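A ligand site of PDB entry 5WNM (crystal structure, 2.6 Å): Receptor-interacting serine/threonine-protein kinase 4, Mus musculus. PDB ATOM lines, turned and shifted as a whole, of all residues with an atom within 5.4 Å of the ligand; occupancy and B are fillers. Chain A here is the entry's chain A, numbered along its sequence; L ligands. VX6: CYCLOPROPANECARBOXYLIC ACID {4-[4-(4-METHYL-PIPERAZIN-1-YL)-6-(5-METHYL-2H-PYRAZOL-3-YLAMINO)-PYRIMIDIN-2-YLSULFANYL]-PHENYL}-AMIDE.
The side-chain carboxylate (OE1) of Glu 69 lies within salt-bridge range of the side-chain amino group (NZ) of Lys 51, at 3.1 Å.
O of Lys 51 sits at hydrogen-bond distance from N of Leu 94 (2.9 Å).
O of Val 36 is in hydrogen-bond range of N of Gly 29 (3.5 Å).
The side-chain carboxylate (OD2) of Asp 161 sits close to the side-chain amide oxygen (OD1) of Asn 148 (3.0 Å).
The backbone carbonyl oxygen (O) of Asn 148 sits at hydrogen-bond distance from the side-chain hydroxyl (OG) of Ser 160, 3.0 Å away.
O of Ala 49 sits at hydrogen-bond distance from N of Met 96.
The backbone carbonyl oxygen of Val 36 lies within hydrogen-bond range of the backbone NH of Val 28 (2.9 Å).
A nitrogen (N20) of the ligand is in hydrogen-bond range of the backbone carbonyl oxygen (O) of Glu 97 (3.3 Å).
N14 of the ligand is in hydrogen-bond range of O of Met 99, at 3.3 Å.
OG of Ser 160 is in hydrogen-bond range of N30 of the ligand (3.3 Å).
The backbone NH (N) of Met 99 lies close to a nitrogen (N20) of the ligand (3.4 Å).
CB of Val 28 touches N13 of the ligand, at 3.7 Å.
Val 36 touches the ligand.
Ala 49 touches the ligand (CB to N19, 3.3 Å).
CD of Lys 51 touches C35 of the ligand, 3.6 Å away.
Glu 69 touches the ligand (OE2 to C34, 3.5 Å).
Leu 82 touches the ligand (CD2 to N19, 3.8 Å).
Met 96 touches the ligand (CE to C21, 3.4 Å).
CE1 of Tyr 98 touches N14 of the ligand (3.4 Å).
Glu 100 touches the ligand (O to C3, 3.1 Å).
O of Thr 101 touches C3 of the ligand (3.7 Å).
Gly 102 touches the ligand (CA to C8, 3.6 Å).
Ala 147 touches the ligand (O to C29, 3.5 Å).
Leu 150 touches the ligand.
Asp 161 touches the ligand.
Hydrophobic or aromatic side chains that line the ligand: Val 28, Val 36, Ala 49, Leu 82, Met 96, Tyr 98, Met 99 and Leu 150.
Of the 23 residues printed, 17 come within 4 Å of the ligand.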
ATOM      1  N   VAL A  28      22.961  21.071   6.449  1.00  0.00           N
ATOM      2  CA  VAL A  28      22.472  19.718   6.757  1.00  0.00           C
ATOM      3  C   VAL A  28      21.633  19.060   5.628  1.00  0.00           C
ATOM      4  O   VAL A  28      21.726  17.846   5.445  1.00  0.00           O
ATOM      5  CB  VAL A  28      21.699  19.654   8.097  1.00  0.00           C
ATOM      6  CG1 VAL A  28      22.655  19.907   9.266  1.00  0.00           C
ATOM      7  CG2 VAL A  28      20.538  20.639   8.141  1.00  0.00           C
ATOM      8  N   GLY A  29      20.835  19.842   4.895  1.00  0.00           N
ATOM      9  CA  GLY A  29      20.013  19.294   3.798  1.00  0.00           C
ATOM     10  C   GLY A  29      20.756  18.916   2.510  1.00  0.00           C
ATOM     11  O   GLY A  29      21.971  18.677   2.539  1.00  0.00           O
ATOM     12  N   VAL A  36      19.126  23.622   3.995  1.00  0.00           N
ATOM     13  CA  VAL A  36      18.782  23.780   5.398  1.00  0.00           C
ATOM     14  C   VAL A  36      20.059  23.890   6.224  1.00  0.00           C
ATOM     15  O   VAL A  36      21.024  23.137   6.012  1.00  0.00           O
ATOM     16  CB  VAL A  36      17.911  22.609   5.898  1.00  0.00           C
ATOM     17  CG1 VAL A  36      17.584  22.746   7.384  1.00  0.00           C
ATOM     18  CG2 VAL A  36      16.632  22.519   5.058  1.00  0.00           C
ATOM     19  N   ALA A  49      16.916  25.503  13.055  1.00  0.00           N
ATOM     20  CA  ALA A  49      17.071  25.084  11.670  1.00  0.00           C
ATOM     21  C   ALA A  49      16.418  26.120  10.757  1.00  0.00           C
ATOM     22  O   ALA A  49      15.294  26.557  11.027  1.00  0.00           O
ATOM     23  CB  ALA A  49      16.438  23.718  11.436  1.00  0.00           C
ATOM     24  N   LYS A  51      15.538  26.766   6.661  1.00  0.00           N
ATOM     25  CA  LYS A  51      15.444  26.324   5.263  1.00  0.00           C
ATOM     26  C   LYS A  51      15.394  27.563   4.376  1.00  0.00           C
ATOM     27  O   LYS A  51      14.440  28.334   4.442  1.00  0.00           O
ATOM     28  CB  LYS A  51      14.167  25.490   5.046  1.00  0.00           C
ATOM     29  CG  LYS A  51      14.044  24.818   3.681  1.00  0.00           C
ATOM     30  CD  LYS A  51      12.588  24.631   3.233  1.00  0.00           C
ATOM     31  CE  LYS A  51      12.037  25.834   2.488  1.00  0.00           C
ATOM     32  NZ  LYS A  51      10.610  25.640   2.135  1.00  0.00           N
ATOM     33  N   GLU A  69       3.349  27.719   4.456  1.00  0.00           N
ATOM     34  CA  GLU A  69       4.017  26.553   5.053  1.00  0.00           C
ATOM     35  C   GLU A  69       4.225  26.762   6.551  1.00  0.00           C
ATOM     36  O   GLU A  69       3.992  25.850   7.345  1.00  0.00           O
ATOM     37  CB  GLU A  69       5.364  26.288   4.375  1.00  0.00           C
ATOM     38  CG  GLU A  69       5.987  24.955   4.790  1.00  0.00           C
ATOM     39  CD  GLU A  69       7.311  24.656   4.110  1.00  0.00           C
ATOM     40  OE1 GLU A  69       7.662  25.330   3.123  1.00  0.00           O
ATOM     41  OE2 GLU A  69       8.006  23.724   4.588  1.00  0.00           O
ATOM     42  N   LEU A  82       7.113  18.990  14.002  1.00  0.00           N
ATOM     43  CA  LEU A  82       8.234  19.930  14.165  1.00  0.00           C
ATOM     44  C   LEU A  82       7.715  21.323  14.494  1.00  0.00           C
ATOM     45  O   LEU A  82       6.849  21.849  13.775  1.00  0.00           O
ATOM     46  CB  LEU A  82       9.085  19.987  12.883  1.00  0.00           C
ATOM     47  CG  LEU A  82      10.390  20.793  12.943  1.00  0.00           C
ATOM     48  CD1 LEU A  82      11.380  20.195  13.934  1.00  0.00           C
ATOM     49  CD2 LEU A  82      11.007  20.886  11.560  1.00  0.00           C
ATOM     50  N   LEU A  94      12.696  29.820   6.284  1.00  0.00           N
ATOM     51  CA  LEU A  94      11.756  29.377   7.306  1.00  0.00           C
ATOM     52  C   LEU A  94      12.542  28.908   8.532  1.00  0.00           C
ATOM     53  O   LEU A  94      13.413  28.045   8.411  1.00  0.00           O
ATOM     54  CB  LEU A  94      10.916  28.232   6.732  1.00  0.00           C
ATOM     55  CG  LEU A  94       9.781  27.639   7.553  1.00  0.00           C
ATOM     56  CD1 LEU A  94       8.643  28.626   7.689  1.00  0.00           C
ATOM     57  CD2 LEU A  94       9.315  26.360   6.884  1.00  0.00           C
ATOM     58  N   MET A  96      12.905  27.121  12.135  1.00  0.00           N
ATOM     59  CA  MET A  96      12.280  25.981  12.846  1.00  0.00           C
ATOM     60  C   MET A  96      13.170  25.396  13.941  1.00  0.00           C
ATOM     61  O   MET A  96      14.349  25.733  14.048  1.00  0.00           O
ATOM     62  CB  MET A  96      11.954  24.874  11.837  1.00  0.00           C
ATOM     63  CG  MET A  96      11.049  25.291  10.697  1.00  0.00           C
ATOM     64  SD  MET A  96      11.129  24.130   9.327  1.00  0.00           S
ATOM     65  CE  MET A  96      12.757  24.489   8.695  1.00  0.00           C
ATOM     66  N   GLU A  97      12.590  24.490  14.729  1.00  0.00           N
ATOM     67  CA  GLU A  97      13.336  23.765  15.745  1.00  0.00           C
ATOM     68  C   GLU A  97      14.440  22.918  15.113  1.00  0.00           C
ATOM     69  O   GLU A  97      14.238  22.382  14.012  1.00  0.00           O
ATOM     70  CB  GLU A  97      12.402  22.864  16.568  1.00  0.00           C
ATOM     71  CG  GLU A  97      12.969  22.388  17.894  1.00  0.00           C
ATOM     72  CD  GLU A  97      13.194  23.537  18.876  1.00  0.00           C
ATOM     73  OE1 GLU A  97      12.228  23.903  19.586  1.00  0.00           O
ATOM     74  OE2 GLU A  97      14.335  24.072  18.943  1.00  0.00           O
ATOM     75  N   TYR A  98      15.589  22.827  15.778  1.00  0.00           N
ATOM     76  CA  TYR A  98      16.673  21.961  15.344  1.00  0.00           C
ATOM     77  C   TYR A  98      16.603  20.644  16.086  1.00  0.00           C
ATOM     78  O   TYR A  98      16.462  20.620  17.294  1.00  0.00           O
ATOM     79  CB  TYR A  98      18.064  22.598  15.550  1.00  0.00           C
ATOM     80  CG  TYR A  98      19.197  21.750  14.991  1.00  0.00           C
ATOM     81  CD1 TYR A  98      19.269  21.447  13.627  1.00  0.00           C
ATOM     82  CD2 TYR A  98      20.185  21.218  15.814  1.00  0.00           C
ATOM     83  CE1 TYR A  98      20.283  20.643  13.119  1.00  0.00           C
ATOM     84  CE2 TYR A  98      21.203  20.422  15.317  1.00  0.00           C
ATOM     85  CZ  TYR A  98      21.241  20.139  13.971  1.00  0.00           C
ATOM     86  OH  TYR A  98      22.267  19.344  13.497  1.00  0.00           O
ATOM     87  N   MET A  99      16.785  19.573  15.330  1.00  0.00           N
ATOM     88  CA  MET A  99      16.665  18.216  15.808  1.00  0.00           C
ATOM     89  C   MET A  99      18.048  17.616  15.612  1.00  0.00           C
ATOM     90  O   MET A  99      18.538  17.556  14.485  1.00  0.00           O
ATOM     91  CB  MET A  99      15.625  17.478  14.965  1.00  0.00           C
ATOM     92  CG  MET A  99      14.217  18.053  15.050  1.00  0.00           C
ATOM     93  SD  MET A  99      13.449  17.747  16.659  1.00  0.00           S
ATOM     94  CE  MET A  99      12.982  16.043  16.461  1.00  0.00           C
ATOM     95  N   GLU A 100      18.684  17.188  16.710  1.00  0.00           N
ATOM     96  CA  GLU A 100      20.103  16.811  16.685  1.00  0.00           C
ATOM     97  C   GLU A 100      20.444  15.588  15.831  1.00  0.00           C
ATOM     98  O   GLU A 100      21.504  15.546  15.221  1.00  0.00           O
ATOM     99  CB  GLU A 100      20.636  16.578  18.105  1.00  0.00           C
ATOM    100  CG  GLU A 100      20.687  17.835  18.973  1.00  0.00           C
ATOM    101  CD  GLU A 100      21.416  17.617  20.295  1.00  0.00           C
ATOM    102  OE1 GLU A 100      22.130  16.598  20.452  1.00  0.00           O
ATOM    103  OE2 GLU A 100      21.266  18.473  21.197  1.00  0.00           O
ATOM    104  N   THR A 101      19.553  14.594  15.801  1.00  0.00           N
ATOM    105  CA  THR A 101      19.878  13.339  15.105  1.00  0.00           C
ATOM    106  C   THR A 101      19.604  13.413  13.600  1.00  0.00           C
ATOM    107  O   THR A 101      20.346  12.829  12.816  1.00  0.00           O
ATOM    108  CB  THR A 101      19.173  12.135  15.757  1.00  0.00           C
ATOM    109  OG1 THR A 101      19.506  12.079  17.152  1.00  0.00           O
ATOM    110  CG2 THR A 101      19.611  10.825  15.094  1.00  0.00           C
ATOM    111  N   GLY A 102      18.558  14.131  13.188  1.00  0.00           N
ATOM    112  CA  GLY A 102      18.293  14.371  11.768  1.00  0.00           C
ATOM    113  C   GLY A 102      17.267  13.399  11.195  1.00  0.00           C
ATOM    114  O   GLY A 102      16.394  12.930  11.914  1.00  0.00           O
ATOM    115  N   SER A 103      17.382  13.108   9.906  1.00  0.00           N
ATOM    116  CA  SER A 103      16.357  12.356   9.197  1.00  0.00           C
ATOM    117  C   SER A 103      16.397  10.870   9.533  1.00  0.00           C
ATOM    118  O   SER A 103      17.424  10.324   9.936  1.00  0.00           O
ATOM    119  CB  SER A 103      16.480  12.539   7.676  1.00  0.00           C
ATOM    120  OG  SER A 103      17.606  11.872   7.143  1.00  0.00           O
ATOM    121  N   LYS A 106      18.742   9.049   6.869  1.00  0.00           N
ATOM    122  CA  LYS A 106      20.142   8.946   7.287  1.00  0.00           C
ATOM    123  C   LYS A 106      20.303   7.861   8.357  1.00  0.00           C
ATOM    124  O   LYS A 106      21.219   7.047   8.265  1.00  0.00           O
ATOM    125  CB  LYS A 106      20.709  10.284   7.791  1.00  0.00           C
ATOM    126  CG  LYS A 106      22.239  10.331   7.806  1.00  0.00           C
ATOM    127  CD  LYS A 106      22.819  11.273   8.855  1.00  0.00           C
ATOM    128  N   ALA A 147      13.034  10.961   4.595  1.00  0.00           N
ATOM    129  CA  ALA A 147      13.757  12.240   4.563  1.00  0.00           C
ATOM    130  C   ALA A 147      13.083  13.377   5.355  1.00  0.00           C
ATOM    131  O   ALA A 147      13.766  14.286   5.807  1.00  0.00           O
ATOM    132  CB  ALA A 147      13.987  12.679   3.115  1.00  0.00           C
ATOM    133  N   ASN A 148      11.763  13.323   5.493  1.00  0.00           N
ATOM    134  CA  ASN A 148      10.960  14.294   6.245  1.00  0.00           C
ATOM    135  C   ASN A 148      10.816  13.994   7.723  1.00  0.00           C
ATOM    136  O   ASN A 148      10.465  14.888   8.493  1.00  0.00           O
ATOM    137  CB  ASN A 148       9.511  14.325   5.716  1.00  0.00           C
ATOM    138  CG  ASN A 148       9.406  14.824   4.300  1.00  0.00           C
ATOM    139  OD1 ASN A 148      10.335  15.435   3.749  1.00  0.00           O
ATOM    140  ND2 ASN A 148       8.249  14.610   3.708  1.00  0.00           N
ATOM    141  N   LEU A 150      11.935  13.549  11.180  1.00  0.00           N
ATOM    142  CA  LEU A 150      13.083  14.001  11.970  1.00  0.00           C
ATOM    143  C   LEU A 150      13.114  13.310  13.336  1.00  0.00           C
ATOM    144  O   LEU A 150      12.087  12.888  13.850  1.00  0.00           O
ATOM    145  CB  LEU A 150      13.042  15.521  12.127  1.00  0.00           C
ATOM    146  CG  LEU A 150      13.365  16.330  10.858  1.00  0.00           C
ATOM    147  CD1 LEU A 150      12.959  17.791  10.981  1.00  0.00           C
ATOM    148  CD2 LEU A 150      14.841  16.237  10.536  1.00  0.00           C
ATOM    149  N   SER A 160       8.018  16.640   9.651  1.00  0.00           N
ATOM    150  CA  SER A 160       8.273  17.927   9.024  1.00  0.00           C
ATOM    151  C   SER A 160       7.920  17.889   7.541  1.00  0.00           C
ATOM    152  O   SER A 160       7.356  16.902   7.054  1.00  0.00           O
ATOM    153  CB  SER A 160       9.741  18.330   9.235  1.00  0.00           C
ATOM    154  OG  SER A 160      10.574  17.831   8.204  1.00  0.00           O
ATOM    155  N   ASP A 161       8.254  18.983   6.850  1.00  0.00           N
ATOM    156  CA  ASP A 161       7.934  19.207   5.436  1.00  0.00           C
ATOM    157  C   ASP A 161       6.445  19.353   5.206  1.00  0.00           C
ATOM    158  O   ASP A 161       5.770  18.417   4.771  1.00  0.00           O
ATOM    159  CB  ASP A 161       8.593  18.157   4.521  1.00  0.00           C
ATOM    160  CG  ASP A 161       8.870  18.703   3.104  1.00  0.00           C
ATOM    161  OD1 ASP A 161       8.351  19.790   2.746  1.00  0.00           O
ATOM    162  OD2 ASP A 161       9.629  18.048   2.347  1.00  0.00           O
ATOM    163  N   PHE A 162       5.956  20.560   5.486  1.00  0.00           N
ATOM    164  CA  PHE A 162       4.568  20.969   5.188  1.00  0.00           C
ATOM    165  C   PHE A 162       4.431  21.844   3.922  1.00  0.00           C
ATOM    166  O   PHE A 162       3.377  22.456   3.702  1.00  0.00           O
ATOM    167  CB  PHE A 162       3.981  21.678   6.427  1.00  0.00           C
ATOM    168  CG  PHE A 162       3.674  20.731   7.562  1.00  0.00           C
ATOM    169  CD1 PHE A 162       4.671  20.327   8.444  1.00  0.00           C
ATOM    170  CD2 PHE A 162       2.390  20.227   7.731  1.00  0.00           C
ATOM    171  CE1 PHE A 162       4.384  19.454   9.479  1.00  0.00           C
ATOM    172  CE2 PHE A 162       2.099  19.346   8.756  1.00  0.00           C
ATOM    173  CZ  PHE A 162       3.105  18.963   9.637  1.00  0.00           C
HETATM  174  N1  VX6 L   1      24.209  14.918  11.618  1.00  0.00           N
HETATM  175  C2  VX6 L   1      23.582  15.930  12.474  1.00  0.00           C
HETATM  176  C3  VX6 L   1      22.093  16.008  12.212  1.00  0.00           C
HETATM  177  N4  VX6 L   1      21.800  16.265  10.791  1.00  0.00           N
HETATM  178  C5  VX6 L   1      22.507  15.336   9.906  1.00  0.00           C
HETATM  179  C6  VX6 L   1      23.989  15.285  10.216  1.00  0.00           C
HETATM  180  C7  VX6 L   1      25.636  14.778  11.923  1.00  0.00           C
HETATM  181  C8  VX6 L   1      20.563  16.781  10.410  1.00  0.00           C
HETATM  182  C9  VX6 L   1      19.802  17.630  11.246  1.00  0.00           C
HETATM  183  C10 VX6 L   1      18.593  18.109  10.752  1.00  0.00           C
HETATM  184  N11 VX6 L   1      18.157  17.778   9.526  1.00  0.00           N
HETATM  185  C12 VX6 L   1      18.932  16.982   8.793  1.00  0.00           C
HETATM  186  N13 VX6 L   1      20.099  16.466   9.184  1.00  0.00           N
HETATM  187  N14 VX6 L   1      17.785  18.943  11.543  1.00  0.00           N
HETATM  188  C15 VX6 L   1      16.639  19.678  11.214  1.00  0.00           C
HETATM  189  C17 VX6 L   1      16.110  19.989   9.975  1.00  0.00           C
HETATM  190  C18 VX6 L   1      14.966  20.752  10.214  1.00  0.00           C
HETATM  191  N19 VX6 L   1      14.793  20.907  11.524  1.00  0.00           N
HETATM  192  N20 VX6 L   1      15.819  20.247  12.123  1.00  0.00           N
HETATM  193  C21 VX6 L   1      13.999  21.350   9.241  1.00  0.00           C
HETATM  194  S23 VX6 L   1      18.362  16.553   7.168  1.00  0.00           S
HETATM  195  C24 VX6 L   1      16.811  17.391   6.949  1.00  0.00           C
HETATM  196  C25 VX6 L   1      16.730  18.646   6.368  1.00  0.00           C
HETATM  197  C26 VX6 L   1      15.502  19.281   6.227  1.00  0.00           C
HETATM  198  C27 VX6 L   1      14.339  18.668   6.651  1.00  0.00           C
HETATM  199  C28 VX6 L   1      14.419  17.399   7.234  1.00  0.00           C
HETATM  200  C29 VX6 L   1      15.641  16.771   7.372  1.00  0.00           C
HETATM  201  N30 VX6 L   1      13.048  19.261   6.539  1.00  0.00           N
HETATM  202  C31 VX6 L   1      12.728  20.405   5.876  1.00  0.00           C
HETATM  203  O32 VX6 L   1      13.274  20.743   4.838  1.00  0.00           O
HETATM  204  C33 VX6 L   1      11.665  21.191   6.508  1.00  0.00           C
HETATM  205  C34 VX6 L   1      10.432  21.479   5.694  1.00  0.00           C
HETATM  206  C35 VX6 L   1      11.390  22.564   5.944  1.00  0.00           C
